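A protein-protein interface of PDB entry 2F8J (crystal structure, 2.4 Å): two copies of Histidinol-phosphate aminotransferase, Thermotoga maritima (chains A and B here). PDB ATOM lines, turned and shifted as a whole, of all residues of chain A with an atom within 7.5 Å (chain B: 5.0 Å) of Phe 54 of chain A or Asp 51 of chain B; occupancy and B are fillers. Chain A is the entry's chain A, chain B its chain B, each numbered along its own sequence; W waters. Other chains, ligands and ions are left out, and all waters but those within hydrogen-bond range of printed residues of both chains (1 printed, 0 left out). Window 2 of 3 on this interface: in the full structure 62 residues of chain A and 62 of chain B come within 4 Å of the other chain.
Val 50 of chain A touches Phe 54 of chain B. Phe 54 of chain A touches Asp 51 of chain B (CE1 to OD1, 3.2 Å). CB of Phe 54 of chain A touches CD2 of Phe 54 of chain B (3.6 Å). CG1 of Val 50 of chain B touches CD2 of Leu 57 of chain A, at 3.96 Å. CD2 of Leu 57 of chain A touches CE1 of Phe 54 of chain B, at 3.4 Å.
Printed residues of chain B within 4 Å of Val 50 of chain A: Phe 54 (3.8 Å). Phe 54 of chain A touches just these residues of chain B: Asp 51 and Phe 54. Arg 56 of chain A touches none of the printed residues of chain B. Of the printed residues of chain B, Leu 57 of chain A touches Val 50 and Phe 54. Printed residues of chain A within 4 Å of Phe 54 of chain B: Val 50, Phe 54 and Leu 57. The nearest residue of chain B that does not touch Phe 54 of chain A is Val 50 of chain B (4.1 Å). The nearest residue of chain A that does not touch Asp 51 of chain B is Leu 57 of chain A (7.4 Å).
Hydrophobic or aromatic side chains of chain A that line the printed part of chain B: Val 50, Phe 54 and Leu 57. Among the printed residues, no Asp or Glu carboxylate lies within 4 Å of a Lys or Arg side-chain nitrogen of the other chain.
Val 50 of chain A touches Phe 54 of chain B, but with the chains exchanged Phe 54 of chain A does not touch Val 50 of chain B (4.1 Å). Phe 54 of chain A touches Asp 51 of chain B, but with the chains exchanged Asp 51 of chain A does not touch Phe 54 of chain B (5.7 Å). Phe 54 of chain B touches its own counterpart, Phe 54 of chain A. 8 positions are printed for both chains. Of the 5 pairs that touch across the chains among the printed residues, 1 has its exchanged pair printed and touching as well.
Water W1 lies within hydrogen-bond range of the side-chain carboxylate of Glu 47 of chain B (2.4 Å) and the backbone carbonyl oxygen of Leu 57 of chain A (3.4 Å).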
ATOM      1  N   ASP A  48       0.136  17.301  -5.540  1.00  0.00           N
ATOM      2  CA  ASP A  48      -0.317  18.580  -5.018  1.00  0.00           C
ATOM      3  C   ASP A  48       0.425  19.759  -5.646  1.00  0.00           C
ATOM      4  O   ASP A  48      -0.166  20.808  -5.909  1.00  0.00           O
ATOM      5  CB  ASP A  48      -0.126  18.603  -3.501  1.00  0.00           C
ATOM      6  CG  ASP A  48      -0.974  17.535  -2.788  1.00  0.00           C
ATOM      7  OD1 ASP A  48      -1.940  17.018  -3.417  1.00  0.00           O
ATOM      8  OD2 ASP A  48      -0.676  17.208  -1.611  1.00  0.00           O
ATOM      9  N   LEU A  49       1.729  19.571  -5.863  1.00  0.00           N
ATOM     10  CA  LEU A  49       2.572  20.598  -6.432  1.00  0.00           C
ATOM     11  C   LEU A  49       2.410  20.724  -7.929  1.00  0.00           C
ATOM     12  O   LEU A  49       2.595  21.810  -8.469  1.00  0.00           O
ATOM     13  CB  LEU A  49       4.033  20.333  -6.072  1.00  0.00           C
ATOM     14  CG  LEU A  49       4.256  20.255  -4.559  1.00  0.00           C
ATOM     15  CD1 LEU A  49       5.735  20.282  -4.269  1.00  0.00           C
ATOM     16  CD2 LEU A  49       3.535  21.377  -3.819  1.00  0.00           C
ATOM     17  N   VAL A  50       2.087  19.621  -8.607  1.00  0.00           N
ATOM     18  CA  VAL A  50       1.742  19.683 -10.027  1.00  0.00           C
ATOM     19  C   VAL A  50       0.474  20.514 -10.226  1.00  0.00           C
ATOM     20  O   VAL A  50       0.396  21.344 -11.147  1.00  0.00           O
ATOM     21  CB  VAL A  50       1.495  18.299 -10.658  1.00  0.00           C
ATOM     22  CG1 VAL A  50       0.969  18.439 -12.112  1.00  0.00           C
ATOM     23  CG2 VAL A  50       2.753  17.463 -10.638  1.00  0.00           C
ATOM     24  N   ASP A  51      -0.522  20.286  -9.376  1.00  0.00           N
ATOM     25  CA  ASP A  51      -1.771  21.047  -9.424  1.00  0.00           C
ATOM     26  C   ASP A  51      -1.548  22.515  -9.064  1.00  0.00           C
ATOM     27  O   ASP A  51      -2.183  23.404  -9.639  1.00  0.00           O
ATOM     28  CB  ASP A  51      -2.807  20.443  -8.473  1.00  0.00           C
ATOM     29  CG  ASP A  51      -3.216  19.012  -8.855  1.00  0.00           C
ATOM     30  OD1 ASP A  51      -2.764  18.479  -9.904  1.00  0.00           O
ATOM     31  OD2 ASP A  51      -4.009  18.415  -8.082  1.00  0.00           O
ATOM     32  N   GLU A  52      -0.657  22.776  -8.110  1.00  0.00           N
ATOM     33  CA  GLU A  52      -0.288  24.157  -7.811  1.00  0.00           C
ATOM     34  C   GLU A  52       0.330  24.872  -8.997  1.00  0.00           C
ATOM     35  O   GLU A  52       0.035  26.041  -9.233  1.00  0.00           O
ATOM     36  CB  GLU A  52       0.690  24.249  -6.669  1.00  0.00           C
ATOM     37  CG  GLU A  52       0.861  25.710  -6.238  1.00  0.00           C
ATOM     38  CD  GLU A  52       1.696  25.850  -5.003  1.00  0.00           C
ATOM     39  OE1 GLU A  52       1.597  24.965  -4.118  1.00  0.00           O
ATOM     40  OE2 GLU A  52       2.450  26.843  -4.923  1.00  0.00           O
ATOM     41  N   VAL A  53       1.212  24.180  -9.722  1.00  0.00           N
ATOM     42  CA  VAL A  53       1.773  24.727 -10.951  1.00  0.00           C
ATOM     43  C   VAL A  53       0.658  25.051 -11.956  1.00  0.00           C
ATOM     44  O   VAL A  53       0.652  26.147 -12.519  1.00  0.00           O
ATOM     45  CB  VAL A  53       2.789  23.770 -11.584  1.00  0.00           C
ATOM     46  CG1 VAL A  53       3.040  24.151 -13.058  1.00  0.00           C
ATOM     47  CG2 VAL A  53       4.099  23.745 -10.761  1.00  0.00           C
ATOM     48  N   PHE A  54      -0.267  24.101 -12.173  1.00  0.00           N
ATOM     49  CA  PHE A  54      -1.394  24.277 -13.117  1.00  0.00           C
ATOM     50  C   PHE A  54      -2.234  25.490 -12.706  1.00  0.00           C
ATOM     51  O   PHE A  54      -2.648  26.285 -13.544  1.00  0.00           O
ATOM     52  CB  PHE A  54      -2.258  22.990 -13.194  1.00  0.00           C
ATOM     53  CG  PHE A  54      -3.661  23.199 -13.792  1.00  0.00           C
ATOM     54  CD1 PHE A  54      -3.848  23.301 -15.170  1.00  0.00           C
ATOM     55  CD2 PHE A  54      -4.782  23.285 -12.973  1.00  0.00           C
ATOM     56  CE1 PHE A  54      -5.116  23.506 -15.719  1.00  0.00           C
ATOM     57  CE2 PHE A  54      -6.056  23.481 -13.517  1.00  0.00           C
ATOM     58  CZ  PHE A  54      -6.215  23.591 -14.897  1.00  0.00           C
ATOM     59  N   ARG A  55      -2.442  25.624 -11.400  1.00  0.00           N
ATOM     60  CA  ARG A  55      -3.205  26.728 -10.780  1.00  0.00           C
ATOM     61  C   ARG A  55      -2.579  28.130 -10.989  1.00  0.00           C
ATOM     62  O   ARG A  55      -3.276  29.096 -11.304  1.00  0.00           O
ATOM     63  CB  ARG A  55      -3.316  26.407  -9.285  1.00  0.00           C
ATOM     64  CG  ARG A  55      -4.240  27.253  -8.465  1.00  0.00           C
ATOM     65  CD  ARG A  55      -4.437  26.625  -7.083  1.00  0.00           C
ATOM     66  NE  ARG A  55      -4.864  25.218  -7.182  1.00  0.00           N
ATOM     67  CZ  ARG A  55      -4.291  24.172  -6.570  1.00  0.00           C
ATOM     68  NH1 ARG A  55      -3.246  24.322  -5.754  1.00  0.00           N
ATOM     69  NH2 ARG A  55      -4.786  22.950  -6.767  1.00  0.00           N
ATOM     70  N   ARG A  56      -1.263  28.218 -10.816  1.00  0.00           N
ATOM     71  CA  ARG A  56      -0.501  29.456 -10.998  1.00  0.00           C
ATOM     72  C   ARG A  56      -0.267  29.836 -12.486  1.00  0.00           C
ATOM     73  O   ARG A  56       0.178  30.948 -12.805  1.00  0.00           O
ATOM     74  CB  ARG A  56       0.836  29.338 -10.238  1.00  0.00           C
ATOM     75  CG  ARG A  56       0.663  29.311  -8.699  1.00  0.00           C
ATOM     76  CD  ARG A  56       1.962  29.039  -7.907  1.00  0.00           C
ATOM     77  NE  ARG A  56       3.024  30.021  -8.158  1.00  0.00           N
ATOM     78  CZ  ARG A  56       4.188  30.096  -7.491  1.00  0.00           C
ATOM     79  NH1 ARG A  56       4.475  29.250  -6.498  1.00  0.00           N
ATOM     80  NH2 ARG A  56       5.073  31.045  -7.814  1.00  0.00           N
ATOM     81  N   LEU A  57      -0.602  28.922 -13.386  1.00  0.00           N
ATOM     82  CA  LEU A  57      -0.239  29.024 -14.789  1.00  0.00           C
ATOM     83  C   LEU A  57      -1.109  30.050 -15.522  1.00  0.00           C
ATOM     84  O   LEU A  57      -2.340  30.015 -15.444  1.00  0.00           O
ATOM     85  CB  LEU A  57      -0.399  27.643 -15.438  1.00  0.00           C
ATOM     86  CG  LEU A  57       0.641  27.119 -16.416  1.00  0.00           C
ATOM     87  CD1 LEU A  57       2.065  27.115 -15.777  1.00  0.00           C
ATOM     88  CD2 LEU A  57       0.240  25.701 -16.835  1.00  0.00           C
ATOM     89  N   ASN A  58      -0.454  30.953 -16.236  1.00  0.00           N
ATOM     90  CA  ASN A  58      -1.114  32.032 -16.955  1.00  0.00           C
ATOM     91  C   ASN A  58      -1.023  31.714 -18.451  1.00  0.00           C
ATOM     92  O   ASN A  58       0.082  31.699 -19.029  1.00  0.00           O
ATOM     93  CB  ASN A  58      -0.438  33.370 -16.613  1.00  0.00           C
ATOM     94  CG  ASN A  58      -1.135  34.579 -17.247  1.00  0.00           C
ATOM     95  OD1 ASN A  58      -2.195  34.467 -17.858  1.00  0.00           O
ATOM     96  ND2 ASN A  58      -0.514  35.743 -17.112  1.00  0.00           N
ATOM     97  N   VAL A 248       6.956  26.931 -17.930  1.00  0.00           N
ATOM     98  CA  VAL A 248       6.441  25.895 -17.038  1.00  0.00           C
ATOM     99  C   VAL A 248       7.561  25.222 -16.249  1.00  0.00           C
ATOM    100  O   VAL A 248       7.364  24.911 -15.107  1.00  0.00           O
ATOM    101  CB  VAL A 248       5.598  24.850 -17.802  1.00  0.00           C
ATOM    102  CG1 VAL A 248       5.253  23.645 -16.928  1.00  0.00           C
ATOM    103  CG2 VAL A 248       4.304  25.499 -18.345  1.00  0.00           C
ATOM    104  N   MET A 251       8.208  27.548 -13.483  1.00  0.00           N
ATOM    105  CA  MET A 251       7.124  27.454 -12.486  1.00  0.00           C
ATOM    106  C   MET A 251       7.238  26.202 -11.595  1.00  0.00           C
ATOM    107  O   MET A 251       7.009  26.291 -10.388  1.00  0.00           O
ATOM    108  CB  MET A 251       5.760  27.506 -13.167  1.00  0.00           C
ATOM    109  CG  MET A 251       4.592  27.685 -12.210  1.00  0.00           C
ATOM    110  SD  MET A 251       4.630  29.276 -11.368  1.00  0.00           S
ATOM    111  CE  MET A 251       3.905  30.303 -12.650  1.00  0.00           C
ATOM    112  N   PHE A 252       7.590  25.056 -12.180  1.00  0.00           N
ATOM    113  CA  PHE A 252       7.917  23.826 -11.409  1.00  0.00           C
ATOM    114  C   PHE A 252       9.027  24.048 -10.380  1.00  0.00           C
ATOM    115  O   PHE A 252       8.893  23.653  -9.225  1.00  0.00           O
ATOM    116  CB  PHE A 252       8.288  22.674 -12.351  1.00  0.00           C
ATOM    117  CG  PHE A 252       7.108  21.854 -12.796  1.00  0.00           C
ATOM    118  CD1 PHE A 252       6.482  20.978 -11.906  1.00  0.00           C
ATOM    119  CD2 PHE A 252       6.604  21.966 -14.076  1.00  0.00           C
ATOM    120  CE1 PHE A 252       5.381  20.205 -12.291  1.00  0.00           C
ATOM    121  CE2 PHE A 252       5.501  21.191 -14.490  1.00  0.00           C
ATOM    122  CZ  PHE A 252       4.884  20.312 -13.580  1.00  0.00           C
ATOM    123  N   VAL A 255       7.763  26.430  -7.558  1.00  0.00           N
ATOM    124  CA  VAL A 255       6.858  25.729  -6.655  1.00  0.00           C
ATOM    125  C   VAL A 255       7.614  24.709  -5.765  1.00  0.00           C
ATOM    126  O   VAL A 255       7.300  24.541  -4.587  1.00  0.00           O
ATOM    127  CB  VAL A 255       5.658  25.066  -7.403  1.00  0.00           C
ATOM    128  CG1 VAL A 255       4.823  24.233  -6.449  1.00  0.00           C
ATOM    129  CG2 VAL A 255       4.757  26.133  -8.095  1.00  0.00           C
ATOM    130  N   GLU B  47      -7.326  27.699 -22.957  1.00  0.00           N
ATOM    131  CA  GLU B  47      -7.434  27.173 -21.586  1.00  0.00           C
ATOM    132  C   GLU B  47      -7.829  25.691 -21.545  1.00  0.00           C
ATOM    133  O   GLU B  47      -7.314  24.945 -20.728  1.00  0.00           O
ATOM    134  CB  GLU B  47      -8.457  27.978 -20.756  1.00  0.00           C
ATOM    135  CG  GLU B  47      -7.943  29.307 -20.175  1.00  0.00           C
ATOM    136  CD  GLU B  47      -6.895  29.150 -19.061  1.00  0.00           C
ATOM    137  OE1 GLU B  47      -6.256  28.080 -18.951  1.00  0.00           O
ATOM    138  OE2 GLU B  47      -6.700  30.115 -18.293  1.00  0.00           O
ATOM    139  N   ASP B  48      -8.750  25.296 -22.423  1.00  0.00           N
ATOM    140  CA  ASP B  48      -9.171  23.910 -22.567  1.00  0.00           C
ATOM    141  C   ASP B  48      -7.990  22.970 -22.876  1.00  0.00           C
ATOM    142  O   ASP B  48      -7.956  21.825 -22.422  1.00  0.00           O
ATOM    143  CB  ASP B  48     -10.223  23.775 -23.689  1.00  0.00           C
ATOM    144  CG  ASP B  48     -11.628  24.219 -23.263  1.00  0.00           C
ATOM    145  OD1 ASP B  48     -11.860  24.496 -22.055  1.00  0.00           O
ATOM    146  OD2 ASP B  48     -12.525  24.281 -24.149  1.00  0.00           O
ATOM    147  N   LEU B  49      -7.044  23.457 -23.666  1.00  0.00           N
ATOM    148  CA  LEU B  49      -5.888  22.676 -24.050  1.00  0.00           C
ATOM    149  C   LEU B  49      -4.824  22.683 -22.967  1.00  0.00           C
ATOM    150  O   LEU B  49      -4.071  21.723 -22.852  1.00  0.00           O
ATOM    151  CB  LEU B  49      -5.353  23.166 -25.403  1.00  0.00           C
ATOM    152  CG  LEU B  49      -6.350  23.072 -26.576  1.00  0.00           C
ATOM    153  CD1 LEU B  49      -5.644  23.253 -27.909  1.00  0.00           C
ATOM    154  CD2 LEU B  49      -7.101  21.738 -26.582  1.00  0.00           C
ATOM    155  N   VAL B  50      -4.764  23.734 -22.153  1.00  0.00           N
ATOM    156  CA  VAL B  50      -3.899  23.714 -20.965  1.00  0.00           C
ATOM    157  C   VAL B  50      -4.389  22.624 -20.029  1.00  0.00           C
ATOM    158  O   VAL B  50      -3.587  21.910 -19.418  1.00  0.00           O
ATOM    159  CB  VAL B  50      -3.885  25.078 -20.212  1.00  0.00           C
ATOM    160  CG1 VAL B  50      -3.047  24.990 -18.929  1.00  0.00           C
ATOM    161  CG2 VAL B  50      -3.352  26.187 -21.105  1.00  0.00           C
ATOM    162  N   ASP B  51      -5.711  22.492 -19.929  1.00  0.00           N
ATOM    163  CA  ASP B  51      -6.320  21.476 -19.085  1.00  0.00           C
ATOM    164  C   ASP B  51      -5.994  20.097 -19.625  1.00  0.00           C
ATOM    165  O   ASP B  51      -5.612  19.197 -18.850  1.00  0.00           O
ATOM    166  CB  ASP B  51      -7.842  21.645 -18.981  1.00  0.00           C
ATOM    167  CG  ASP B  51      -8.267  23.001 -18.379  1.00  0.00           C
ATOM    168  OD1 ASP B  51      -7.394  23.782 -17.907  1.00  0.00           O
ATOM    169  OD2 ASP B  51      -9.497  23.283 -18.380  1.00  0.00           O
ATOM    170  N   GLU B  52      -6.134  19.911 -20.935  1.00  0.00           N
ATOM    171  CA  GLU B  52      -5.826  18.611 -21.515  1.00  0.00           C
ATOM    172  C   GLU B  52      -4.357  18.234 -21.269  1.00  0.00           C
ATOM    173  O   GLU B  52      -4.060  17.113 -20.876  1.00  0.00           O
ATOM    174  CB  GLU B  52      -6.152  18.560 -23.005  1.00  0.00           C
ATOM    175  CG  GLU B  52      -5.685  17.245 -23.684  1.00  0.00           C
ATOM    176  CD  GLU B  52      -6.276  17.037 -25.078  1.00  0.00           C
ATOM    177  OE1 GLU B  52      -7.370  17.597 -25.348  1.00  0.00           O
ATOM    178  OE2 GLU B  52      -5.653  16.307 -25.893  1.00  0.00           O
ATOM    179  N   VAL B  53      -3.439  19.165 -21.506  1.00  0.00           N
ATOM    180  CA  VAL B  53      -2.031  18.953 -21.156  1.00  0.00           C
ATOM    181  C   VAL B  53      -1.883  18.346 -19.747  1.00  0.00           C
ATOM    182  O   VAL B  53      -1.213  17.330 -19.584  1.00  0.00           O
ATOM    183  CB  VAL B  53      -1.196  20.260 -21.314  1.00  0.00           C
ATOM    184  CG1 VAL B  53       0.200  20.114 -20.725  1.00  0.00           C
ATOM    185  CG2 VAL B  53      -1.102  20.652 -22.800  1.00  0.00           C
ATOM    186  N   PHE B  54      -2.540  18.932 -18.751  1.00  0.00           N
ATOM    187  CA  PHE B  54      -2.321  18.524 -17.365  1.00  0.00           C
ATOM    188  C   PHE B  54      -3.015  17.230 -16.974  1.00  0.00           C
ATOM    189  O   PHE B  54      -2.561  16.530 -16.053  1.00  0.00           O
ATOM    190  CB  PHE B  54      -2.594  19.681 -16.385  1.00  0.00           C
ATOM    191  CG  PHE B  54      -1.377  20.595 -16.218  1.00  0.00           C
ATOM    192  CD1 PHE B  54      -1.023  21.505 -17.219  1.00  0.00           C
ATOM    193  CD2 PHE B  54      -0.541  20.481 -15.106  1.00  0.00           C
ATOM    194  CE1 PHE B  54       0.115  22.290 -17.095  1.00  0.00           C
ATOM    195  CE2 PHE B  54       0.600  21.280 -14.976  1.00  0.00           C
ATOM    196  CZ  PHE B  54       0.934  22.169 -15.971  1.00  0.00           C
ATOM    197  N   ARG B  55      -4.068  16.861 -17.699  1.00  0.00           N
ATOM    198  CA  ARG B  55      -4.683  15.564 -17.453  1.00  0.00           C
ATOM    199  C   ARG B  55      -4.001  14.455 -18.259  1.00  0.00           C
ATOM    200  O   ARG B  55      -4.369  13.294 -18.151  1.00  0.00           O
ATOM    201  CB  ARG B  55      -6.206  15.603 -17.629  1.00  0.00           C
ATOM    202  CG  ARG B  55      -6.702  15.820 -19.019  1.00  0.00           C
ATOM    203  CD  ARG B  55      -8.225  15.544 -19.097  1.00  0.00           C
ATOM    204  NE  ARG B  55      -9.016  16.706 -18.695  1.00  0.00           N
ATOM    205  CZ  ARG B  55      -9.456  17.653 -19.524  1.00  0.00           C
ATOM    206  NH1 ARG B  55      -9.204  17.601 -20.837  1.00  0.00           N
ATOM    207  NH2 ARG B  55     -10.157  18.671 -19.035  1.00  0.00           N
HETATM  208  O   HOH W   1      -4.449  28.101 -17.322  1.00  0.00           O
